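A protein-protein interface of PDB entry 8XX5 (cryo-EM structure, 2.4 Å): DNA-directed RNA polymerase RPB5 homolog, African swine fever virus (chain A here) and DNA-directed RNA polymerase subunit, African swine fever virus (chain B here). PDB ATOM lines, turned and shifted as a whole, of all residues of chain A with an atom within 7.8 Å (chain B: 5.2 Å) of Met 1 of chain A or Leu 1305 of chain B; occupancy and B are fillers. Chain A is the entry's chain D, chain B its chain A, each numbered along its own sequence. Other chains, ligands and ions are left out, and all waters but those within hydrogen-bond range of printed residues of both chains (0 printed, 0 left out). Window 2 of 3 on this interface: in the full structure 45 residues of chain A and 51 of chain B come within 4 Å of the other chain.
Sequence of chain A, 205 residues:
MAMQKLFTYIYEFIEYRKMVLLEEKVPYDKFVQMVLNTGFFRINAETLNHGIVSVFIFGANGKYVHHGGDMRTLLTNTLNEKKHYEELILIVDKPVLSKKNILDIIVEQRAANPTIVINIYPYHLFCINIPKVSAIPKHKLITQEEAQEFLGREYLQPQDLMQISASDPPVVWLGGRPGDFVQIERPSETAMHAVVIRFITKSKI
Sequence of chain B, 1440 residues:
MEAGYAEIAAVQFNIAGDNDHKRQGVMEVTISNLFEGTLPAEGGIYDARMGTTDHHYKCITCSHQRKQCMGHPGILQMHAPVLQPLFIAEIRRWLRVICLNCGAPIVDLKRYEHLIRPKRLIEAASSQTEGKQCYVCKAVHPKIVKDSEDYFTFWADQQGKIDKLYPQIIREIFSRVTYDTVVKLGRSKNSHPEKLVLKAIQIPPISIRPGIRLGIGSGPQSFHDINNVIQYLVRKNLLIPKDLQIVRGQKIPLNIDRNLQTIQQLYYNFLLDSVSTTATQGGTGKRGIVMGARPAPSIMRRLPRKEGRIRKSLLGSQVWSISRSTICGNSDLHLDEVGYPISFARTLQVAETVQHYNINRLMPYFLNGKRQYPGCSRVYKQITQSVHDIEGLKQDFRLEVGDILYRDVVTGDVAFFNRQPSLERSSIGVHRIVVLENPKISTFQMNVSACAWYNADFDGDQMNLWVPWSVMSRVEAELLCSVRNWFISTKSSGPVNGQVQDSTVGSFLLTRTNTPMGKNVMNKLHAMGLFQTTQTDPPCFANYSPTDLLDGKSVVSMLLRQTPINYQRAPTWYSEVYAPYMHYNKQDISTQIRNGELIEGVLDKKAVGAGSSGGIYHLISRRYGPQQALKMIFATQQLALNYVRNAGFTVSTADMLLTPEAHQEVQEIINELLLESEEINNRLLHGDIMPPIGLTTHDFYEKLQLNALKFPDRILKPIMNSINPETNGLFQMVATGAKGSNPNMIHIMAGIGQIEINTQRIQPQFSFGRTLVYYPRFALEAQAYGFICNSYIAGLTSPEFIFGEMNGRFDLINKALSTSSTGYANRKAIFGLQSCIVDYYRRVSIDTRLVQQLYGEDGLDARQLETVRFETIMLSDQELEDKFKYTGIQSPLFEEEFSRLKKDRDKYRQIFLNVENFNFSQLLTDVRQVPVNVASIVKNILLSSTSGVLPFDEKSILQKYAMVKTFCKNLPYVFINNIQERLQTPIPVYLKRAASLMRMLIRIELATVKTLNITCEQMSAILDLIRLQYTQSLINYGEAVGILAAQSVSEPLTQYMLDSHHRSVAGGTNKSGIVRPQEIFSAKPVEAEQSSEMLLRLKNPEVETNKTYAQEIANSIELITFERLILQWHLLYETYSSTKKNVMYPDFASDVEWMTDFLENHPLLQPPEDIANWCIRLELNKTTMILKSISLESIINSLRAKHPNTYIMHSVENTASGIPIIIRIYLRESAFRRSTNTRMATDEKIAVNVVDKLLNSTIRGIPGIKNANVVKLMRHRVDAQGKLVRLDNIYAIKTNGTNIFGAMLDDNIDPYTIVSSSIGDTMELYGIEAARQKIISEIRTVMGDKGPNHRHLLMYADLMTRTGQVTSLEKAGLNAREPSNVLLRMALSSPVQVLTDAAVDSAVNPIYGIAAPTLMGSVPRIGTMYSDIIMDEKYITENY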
ATOM      1  N   MET A   1       6.669   6.849  21.155  1.00  0.00           N
ATOM      2  CA  MET A   1       7.534   7.933  21.605  1.00  0.00           C
ATOM      3  C   MET A   1       8.799   8.003  20.758  1.00  0.00           C
ATOM      4  O   MET A   1       9.787   8.619  21.155  1.00  0.00           O
ATOM      5  CB  MET A   1       7.900   7.752  23.079  1.00  0.00           C
ATOM      6  CG  MET A   1       6.832   7.054  23.907  1.00  0.00           C
ATOM      7  SD  MET A   1       6.774   7.654  25.605  1.00  0.00           S
ATOM      8  CE  MET A   1       6.153   9.315  25.353  1.00  0.00           C
ATOM      9  N   ALA A   2       8.754   7.365  19.586  1.00  0.00           N
ATOM     10  CA  ALA A   2       9.938   7.286  18.738  1.00  0.00           C
ATOM     11  C   ALA A   2      10.380   8.664  18.265  1.00  0.00           C
ATOM     12  O   ALA A   2      11.580   8.959  18.225  1.00  0.00           O
ATOM     13  CB  ALA A   2       9.667   6.372  17.543  1.00  0.00           C
ATOM     14  N   MET A   3       9.426   9.522  17.904  1.00  0.00           N
ATOM     15  CA  MET A   3       9.783  10.799  17.300  1.00  0.00           C
ATOM     16  C   MET A   3      10.412  11.737  18.326  1.00  0.00           C
ATOM     17  O   MET A   3      11.346  12.478  18.005  1.00  0.00           O
ATOM     18  CB  MET A   3       8.546  11.434  16.663  1.00  0.00           C
ATOM     19  CG  MET A   3       7.975  10.665  15.460  1.00  0.00           C
ATOM     20  SD  MET A   3       9.003  10.294  14.012  1.00  0.00           S
ATOM     21  CE  MET A   3      10.211  11.611  14.003  1.00  0.00           C
ATOM     22  N   GLN A   4       9.922  11.706  19.568  1.00  0.00           N
ATOM     23  CA  GLN A   4      10.509  12.522  20.630  1.00  0.00           C
ATOM     24  C   GLN A   4      11.953  12.121  20.905  1.00  0.00           C
ATOM     25  O   GLN A   4      12.847  12.976  20.986  1.00  0.00           O
ATOM     26  CB  GLN A   4       9.677  12.393  21.906  1.00  0.00           C
ATOM     27  CG  GLN A   4       9.343  13.708  22.575  1.00  0.00           C
ATOM     28  CD  GLN A   4      10.557  14.390  23.177  1.00  0.00           C
ATOM     29  OE1 GLN A   4      11.549  13.739  23.506  1.00  0.00           O
ATOM     30  NE2 GLN A   4      10.483  15.707  23.322  1.00  0.00           N
ATOM     31  N   LYS A   5      12.195  10.819  21.077  1.00  0.00           N
ATOM     32  CA  LYS A   5      13.550  10.347  21.333  1.00  0.00           C
ATOM     33  C   LYS A   5      14.460  10.660  20.157  1.00  0.00           C
ATOM     34  O   LYS A   5      15.610  11.072  20.342  1.00  0.00           O
ATOM     35  CB  LYS A   5      13.539   8.848  21.630  1.00  0.00           C
ATOM     36  CG  LYS A   5      13.122   8.497  23.049  1.00  0.00           C
ATOM     37  CD  LYS A   5      13.596   9.545  24.046  1.00  0.00           C
ATOM     38  CE  LYS A   5      13.217   9.168  25.469  1.00  0.00           C
ATOM     39  NZ  LYS A   5      12.009   8.301  25.514  1.00  0.00           N
ATOM     40  N   LEU A   6      13.954  10.477  18.937  1.00  0.00           N
ATOM     41  CA  LEU A   6      14.718  10.844  17.753  1.00  0.00           C
ATOM     42  C   LEU A   6      15.107  12.314  17.790  1.00  0.00           C
ATOM     43  O   LEU A   6      16.268  12.667  17.563  1.00  0.00           O
ATOM     44  CB  LEU A   6      13.903  10.538  16.500  1.00  0.00           C
ATOM     45  CG  LEU A   6      14.471   9.510  15.532  1.00  0.00           C
ATOM     46  CD1 LEU A   6      13.686   9.570  14.248  1.00  0.00           C
ATOM     47  CD2 LEU A   6      15.935   9.787  15.271  1.00  0.00           C
ATOM     48  N   PHE A   7      14.145  13.187  18.098  1.00  0.00           N
ATOM     49  CA  PHE A   7      14.418  14.618  18.116  1.00  0.00           C
ATOM     50  C   PHE A   7      15.469  14.975  19.157  1.00  0.00           C
ATOM     51  O   PHE A   7      16.370  15.777  18.886  1.00  0.00           O
ATOM     52  CB  PHE A   7      13.130  15.395  18.379  1.00  0.00           C
ATOM     53  CG  PHE A   7      13.344  16.868  18.546  1.00  0.00           C
ATOM     54  CD1 PHE A   7      13.702  17.657  17.467  1.00  0.00           C
ATOM     55  CD2 PHE A   7      13.203  17.462  19.788  1.00  0.00           C
ATOM     56  CE1 PHE A   7      13.906  19.011  17.623  1.00  0.00           C
ATOM     57  CE2 PHE A   7      13.406  18.815  19.950  1.00  0.00           C
ATOM     58  CZ  PHE A   7      13.759  19.590  18.866  1.00  0.00           C
ATOM     59  N   THR A   8      15.372  14.398  20.356  1.00  0.00           N
ATOM     60  CA  THR A   8      16.303  14.796  21.410  1.00  0.00           C
ATOM     61  C   THR A   8      17.684  14.185  21.196  1.00  0.00           C
ATOM     62  O   THR A   8      18.689  14.749  21.645  1.00  0.00           O
ATOM     63  CB  THR A   8      15.766  14.423  22.794  1.00  0.00           C
ATOM     64  OG1 THR A   8      16.792  14.639  23.770  1.00  0.00           O
ATOM     65  CG2 THR A   8      15.368  12.971  22.846  1.00  0.00           C
ATOM     66  N   TYR A  28       9.803  20.859  19.351  1.00  0.00           N
ATOM     67  CA  TYR A  28       9.275  19.524  19.088  1.00  0.00           C
ATOM     68  C   TYR A  28       8.020  19.593  18.224  1.00  0.00           C
ATOM     69  O   TYR A  28       7.880  18.846  17.249  1.00  0.00           O
ATOM     70  CB  TYR A  28       8.962  18.820  20.410  1.00  0.00           C
ATOM     71  CG  TYR A  28       8.424  17.412  20.262  1.00  0.00           C
ATOM     72  CD1 TYR A  28       8.686  16.653  19.129  1.00  0.00           C
ATOM     73  CD2 TYR A  28       7.586  16.871  21.228  1.00  0.00           C
ATOM     74  CE1 TYR A  28       8.181  15.380  18.989  1.00  0.00           C
ATOM     75  CE2 TYR A  28       7.063  15.603  21.088  1.00  0.00           C
ATOM     76  CZ  TYR A  28       7.365  14.858  19.968  1.00  0.00           C
ATOM     77  OH  TYR A  28       6.852  13.590  19.827  1.00  0.00           O
ATOM     78  N   TYR A 123      15.023   3.607  13.209  1.00  0.00           N
ATOM     79  CA  TYR A 123      14.760   4.606  14.239  1.00  0.00           C
ATOM     80  C   TYR A 123      15.554   4.328  15.509  1.00  0.00           C
ATOM     81  O   TYR A 123      16.091   5.256  16.125  1.00  0.00           O
ATOM     82  CB  TYR A 123      13.265   4.667  14.557  1.00  0.00           C
ATOM     83  CG  TYR A 123      12.447   5.436  13.549  1.00  0.00           C
ATOM     84  CD1 TYR A 123      12.977   6.538  12.896  1.00  0.00           C
ATOM     85  CD2 TYR A 123      11.134   5.084  13.277  1.00  0.00           C
ATOM     86  CE1 TYR A 123      12.233   7.254  11.981  1.00  0.00           C
ATOM     87  CE2 TYR A 123      10.380   5.796  12.365  1.00  0.00           C
ATOM     88  CZ  TYR A 123      10.935   6.880  11.721  1.00  0.00           C
ATOM     89  OH  TYR A 123      10.189   7.591  10.811  1.00  0.00           O
ATOM     90  N   HIS A 124      15.646   3.060  15.915  1.00  0.00           N
ATOM     91  CA  HIS A 124      16.253   2.729  17.199  1.00  0.00           C
ATOM     92  C   HIS A 124      17.737   3.056  17.256  1.00  0.00           C
ATOM     93  O   HIS A 124      18.308   3.069  18.352  1.00  0.00           O
ATOM     94  CB  HIS A 124      16.028   1.249  17.528  1.00  0.00           C
ATOM     95  CG  HIS A 124      16.615   0.300  16.530  1.00  0.00           C
ATOM     96  ND1 HIS A 124      17.973   0.159  16.340  1.00  0.00           N
ATOM     97  CD2 HIS A 124      16.025  -0.576  15.682  1.00  0.00           C
ATOM     98  CE1 HIS A 124      18.193  -0.753  15.412  1.00  0.00           C
ATOM     99  NE2 HIS A 124      17.029  -1.214  14.996  1.00  0.00           N
ATOM    100  N   CYS A 127      17.525   6.619  18.818  1.00  0.00           N
ATOM    101  CA  CYS A 127      16.544   6.830  19.872  1.00  0.00           C
ATOM    102  C   CYS A 127      17.150   6.721  21.263  1.00  0.00           C
ATOM    103  O   CYS A 127      16.412   6.737  22.253  1.00  0.00           O
ATOM    104  CB  CYS A 127      15.388   5.840  19.722  1.00  0.00           C
ATOM    105  SG  CYS A 127      14.045   6.444  18.673  1.00  0.00           S
ATOM    106  N   ILE A 128      18.474   6.608  21.355  1.00  0.00           N
ATOM    107  CA  ILE A 128      19.182   6.546  22.627  1.00  0.00           C
ATOM    108  C   ILE A 128      20.607   7.010  22.374  1.00  0.00           C
ATOM    109  O   ILE A 128      21.126   6.903  21.261  1.00  0.00           O
ATOM    110  CB  ILE A 128      19.158   5.121  23.234  1.00  0.00           C
ATOM    111  CG1 ILE A 128      19.738   5.114  24.647  1.00  0.00           C
ATOM    112  CG2 ILE A 128      19.908   4.145  22.344  1.00  0.00           C
ATOM    113  CD1 ILE A 128      19.389   3.882  25.431  1.00  0.00           C
ATOM    114  N   ILE B1300      13.542  -4.148  23.420  1.00  0.00           N
ATOM    115  CA  ILE B1300      14.494  -3.139  23.878  1.00  0.00           C
ATOM    116  C   ILE B1300      14.070  -1.759  23.403  1.00  0.00           C
ATOM    117  O   ILE B1300      14.141  -0.779  24.153  1.00  0.00           O
ATOM    118  CB  ILE B1300      15.921  -3.481  23.409  1.00  0.00           C
ATOM    119  CG1 ILE B1300      16.384  -4.810  24.002  1.00  0.00           C
ATOM    120  CG2 ILE B1300      16.889  -2.381  23.805  1.00  0.00           C
ATOM    121  CD1 ILE B1300      17.699  -5.283  23.434  1.00  0.00           C
ATOM    122  N   PHE B1301      13.626  -1.658  22.150  1.00  0.00           N
ATOM    123  CA  PHE B1301      13.188  -0.373  21.616  1.00  0.00           C
ATOM    124  C   PHE B1301      11.984   0.160  22.386  1.00  0.00           C
ATOM    125  O   PHE B1301      11.969   1.320  22.816  1.00  0.00           O
ATOM    126  CB  PHE B1301      12.865  -0.520  20.129  1.00  0.00           C
ATOM    127  CG  PHE B1301      12.723   0.785  19.407  1.00  0.00           C
ATOM    128  CD1 PHE B1301      13.456   1.887  19.797  1.00  0.00           C
ATOM    129  CD2 PHE B1301      11.860   0.905  18.332  1.00  0.00           C
ATOM    130  CE1 PHE B1301      13.328   3.087  19.133  1.00  0.00           C
ATOM    131  CE2 PHE B1301      11.729   2.102  17.663  1.00  0.00           C
ATOM    132  CZ  PHE B1301      12.466   3.194  18.064  1.00  0.00           C
ATOM    133  N   GLY B1302      10.970  -0.684  22.586  1.00  0.00           N
ATOM    134  CA  GLY B1302       9.800  -0.254  23.332  1.00  0.00           C
ATOM    135  C   GLY B1302      10.119   0.094  24.772  1.00  0.00           C
ATOM    136  O   GLY B1302       9.613   1.081  25.309  1.00  0.00           O
ATOM    137  N   ALA B1303      10.965  -0.712  25.419  1.00  0.00           N
ATOM    138  CA  ALA B1303      11.354  -0.423  26.794  1.00  0.00           C
ATOM    139  C   ALA B1303      12.154   0.869  26.893  1.00  0.00           C
ATOM    140  O   ALA B1303      12.077   1.565  27.910  1.00  0.00           O
ATOM    141  CB  ALA B1303      12.153  -1.588  27.372  1.00  0.00           C
ATOM    142  N   MET B1304      12.924   1.203  25.858  1.00  0.00           N
ATOM    143  CA  MET B1304      13.683   2.446  25.859  1.00  0.00           C
ATOM    144  C   MET B1304      12.843   3.645  25.445  1.00  0.00           C
ATOM    145  O   MET B1304      13.264   4.784  25.670  1.00  0.00           O
ATOM    146  CB  MET B1304      14.900   2.321  24.940  1.00  0.00           C
ATOM    147  CG  MET B1304      14.708   2.905  23.552  1.00  0.00           C
ATOM    148  SD  MET B1304      16.233   2.908  22.593  1.00  0.00           S
ATOM    149  CE  MET B1304      16.913   1.315  23.041  1.00  0.00           C
ATOM    150  N   LEU B1305      11.672   3.420  24.847  1.00  0.00           N
ATOM    151  CA  LEU B1305      10.822   4.544  24.465  1.00  0.00           C
ATOM    152  C   LEU B1305      10.105   5.151  25.666  1.00  0.00           C
ATOM    153  O   LEU B1305       9.941   6.374  25.738  1.00  0.00           O
ATOM    154  CB  LEU B1305       9.810   4.106  23.408  1.00  0.00           C
ATOM    155  CG  LEU B1305      10.413   3.889  22.020  1.00  0.00           C
ATOM    156  CD1 LEU B1305       9.440   3.164  21.101  1.00  0.00           C
ATOM    157  CD2 LEU B1305      10.872   5.204  21.423  1.00  0.00           C
ATOM    158  N   ASP B1306       9.673   4.323  26.612  1.00  0.00           N
ATOM    159  CA  ASP B1306       8.931   4.823  27.761  1.00  0.00           C
ATOM    160  C   ASP B1306       9.893   5.555  28.690  1.00  0.00           C
ATOM    161  O   ASP B1306      11.045   5.152  28.863  1.00  0.00           O
ATOM    162  CB  ASP B1306       8.223   3.660  28.472  1.00  0.00           C
ATOM    163  CG  ASP B1306       7.722   4.000  29.886  1.00  0.00           C
ATOM    164  OD1 ASP B1306       7.902   5.125  30.398  1.00  0.00           O
ATOM    165  OD2 ASP B1306       7.112   3.100  30.501  1.00  0.00           O
ATOM    166  N   ASP B1307       9.407   6.635  29.298  1.00  0.00           N
ATOM    167  CA  ASP B1307      10.234   7.509  30.119  1.00  0.00           C
ATOM    168  C   ASP B1307      10.270   7.108  31.587  1.00  0.00           C
ATOM    169  O   ASP B1307      10.924   7.789  32.382  1.00  0.00           O
ATOM    170  CB  ASP B1307       9.749   8.956  29.995  1.00  0.00           C
ATOM    171  CG  ASP B1307      10.262   9.635  28.743  1.00  0.00           C
ATOM    172  OD1 ASP B1307      11.400  10.151  28.768  1.00  0.00           O
ATOM    173  OD2 ASP B1307       9.530   9.651  27.731  1.00  0.00           O
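The side-chain amino group of Lys 5 of chain A is in salt-bridge range of the side-chain carboxylate of Asp 1307 of chain B, 3.6 Å away. O of Leu 1305 of chain B is in hydrogen-bond range of NZ of Lys 5 of chain A (2.8 Å). O of Leu 1305 of chain B sits close to SD of Met 1 of chain A, at 3.4 Å.
Of the printed residues of chain B, Met 1 of chain A touches Leu 1305. Leu 1305 of chain B touches just these residues of chain A: Met 1 (3.4 Å), Ala 2 (3.5 Å) and Lys 5 (2.8 Å). Of the printed residues of chain B, Tyr 123 of chain A touches Phe 1301 (3.9 Å). Printed residues of chain A within 4 Å of Phe 1301 of chain B: Tyr 123, His 124 and Cys 127. Of the printed residues of chain B, His 124 of chain A touches Phe 1301 (3.5 Å). Gln 4 of chain A touches none of the printed residues of chain B. The nearest residue of chain A that does not touch Leu 1305 of chain B is Cys 127 of chain A (4.4 Å). The nearest printed residue of chain B that does not touch Cys 127 of chain A is Leu 1305 of chain B (4.4 Å).
Among the printed residues, merely in contact across the chains: Cys 127 of chain A with Phe 1301 of chain B (3.5 Å), His 124 of chain A with Phe 1301 of chain B (3.5 Å), Ala 2 of chain A with Leu 1305 of chain B (3.5 Å), Ile 128 of chain A with Met 1304 of chain B (3.7 Å), Lys 5 of chain A with Met 1304 of chain B (3.7 Å), Cys 127 of chain A with Met 1304 of chain B (3.8 Å) and Tyr 123 of chain A with Phe 1301 of chain B (3.9 Å).
Of the 13 printed residues of chain A, 7 touch a printed residue of chain B. Printed residues of chain A that touch a printed residue of chain B: Met 1, Ala 2, Lys 5, Tyr 123, His 124, Cys 127 and Ile 128. Hydrophobic or aromatic side chains of chain A within 4 Å of the printed part of chain B: Met 1, Tyr 123, His 124 and Ile 128. Of the 8 printed residues of chain B, 4 touch a printed residue of chain A. Along chain B the printed residues that touch a printed residue of chain A span positions 1301 to 1307. Among the printed residues, 10 pairs touch across the chains. Among the printed residues, Asp or Glu carboxylates within 4 Å of a Lys or Arg side-chain nitrogen of the other chain: Lys 5 of chain A with Asp 1307 of chain B (3.6 Å).
The backbone carbonyl oxygen (O) of Tyr 123 of chain A sits at hydrogen-bond distance from the side-chain sulfur (SG) of Cys 127 of chain A, 3.5 Å away. O of Ala 2 of chain A lies within hydrogen-bond range of SG of Cys 127 of chain A.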
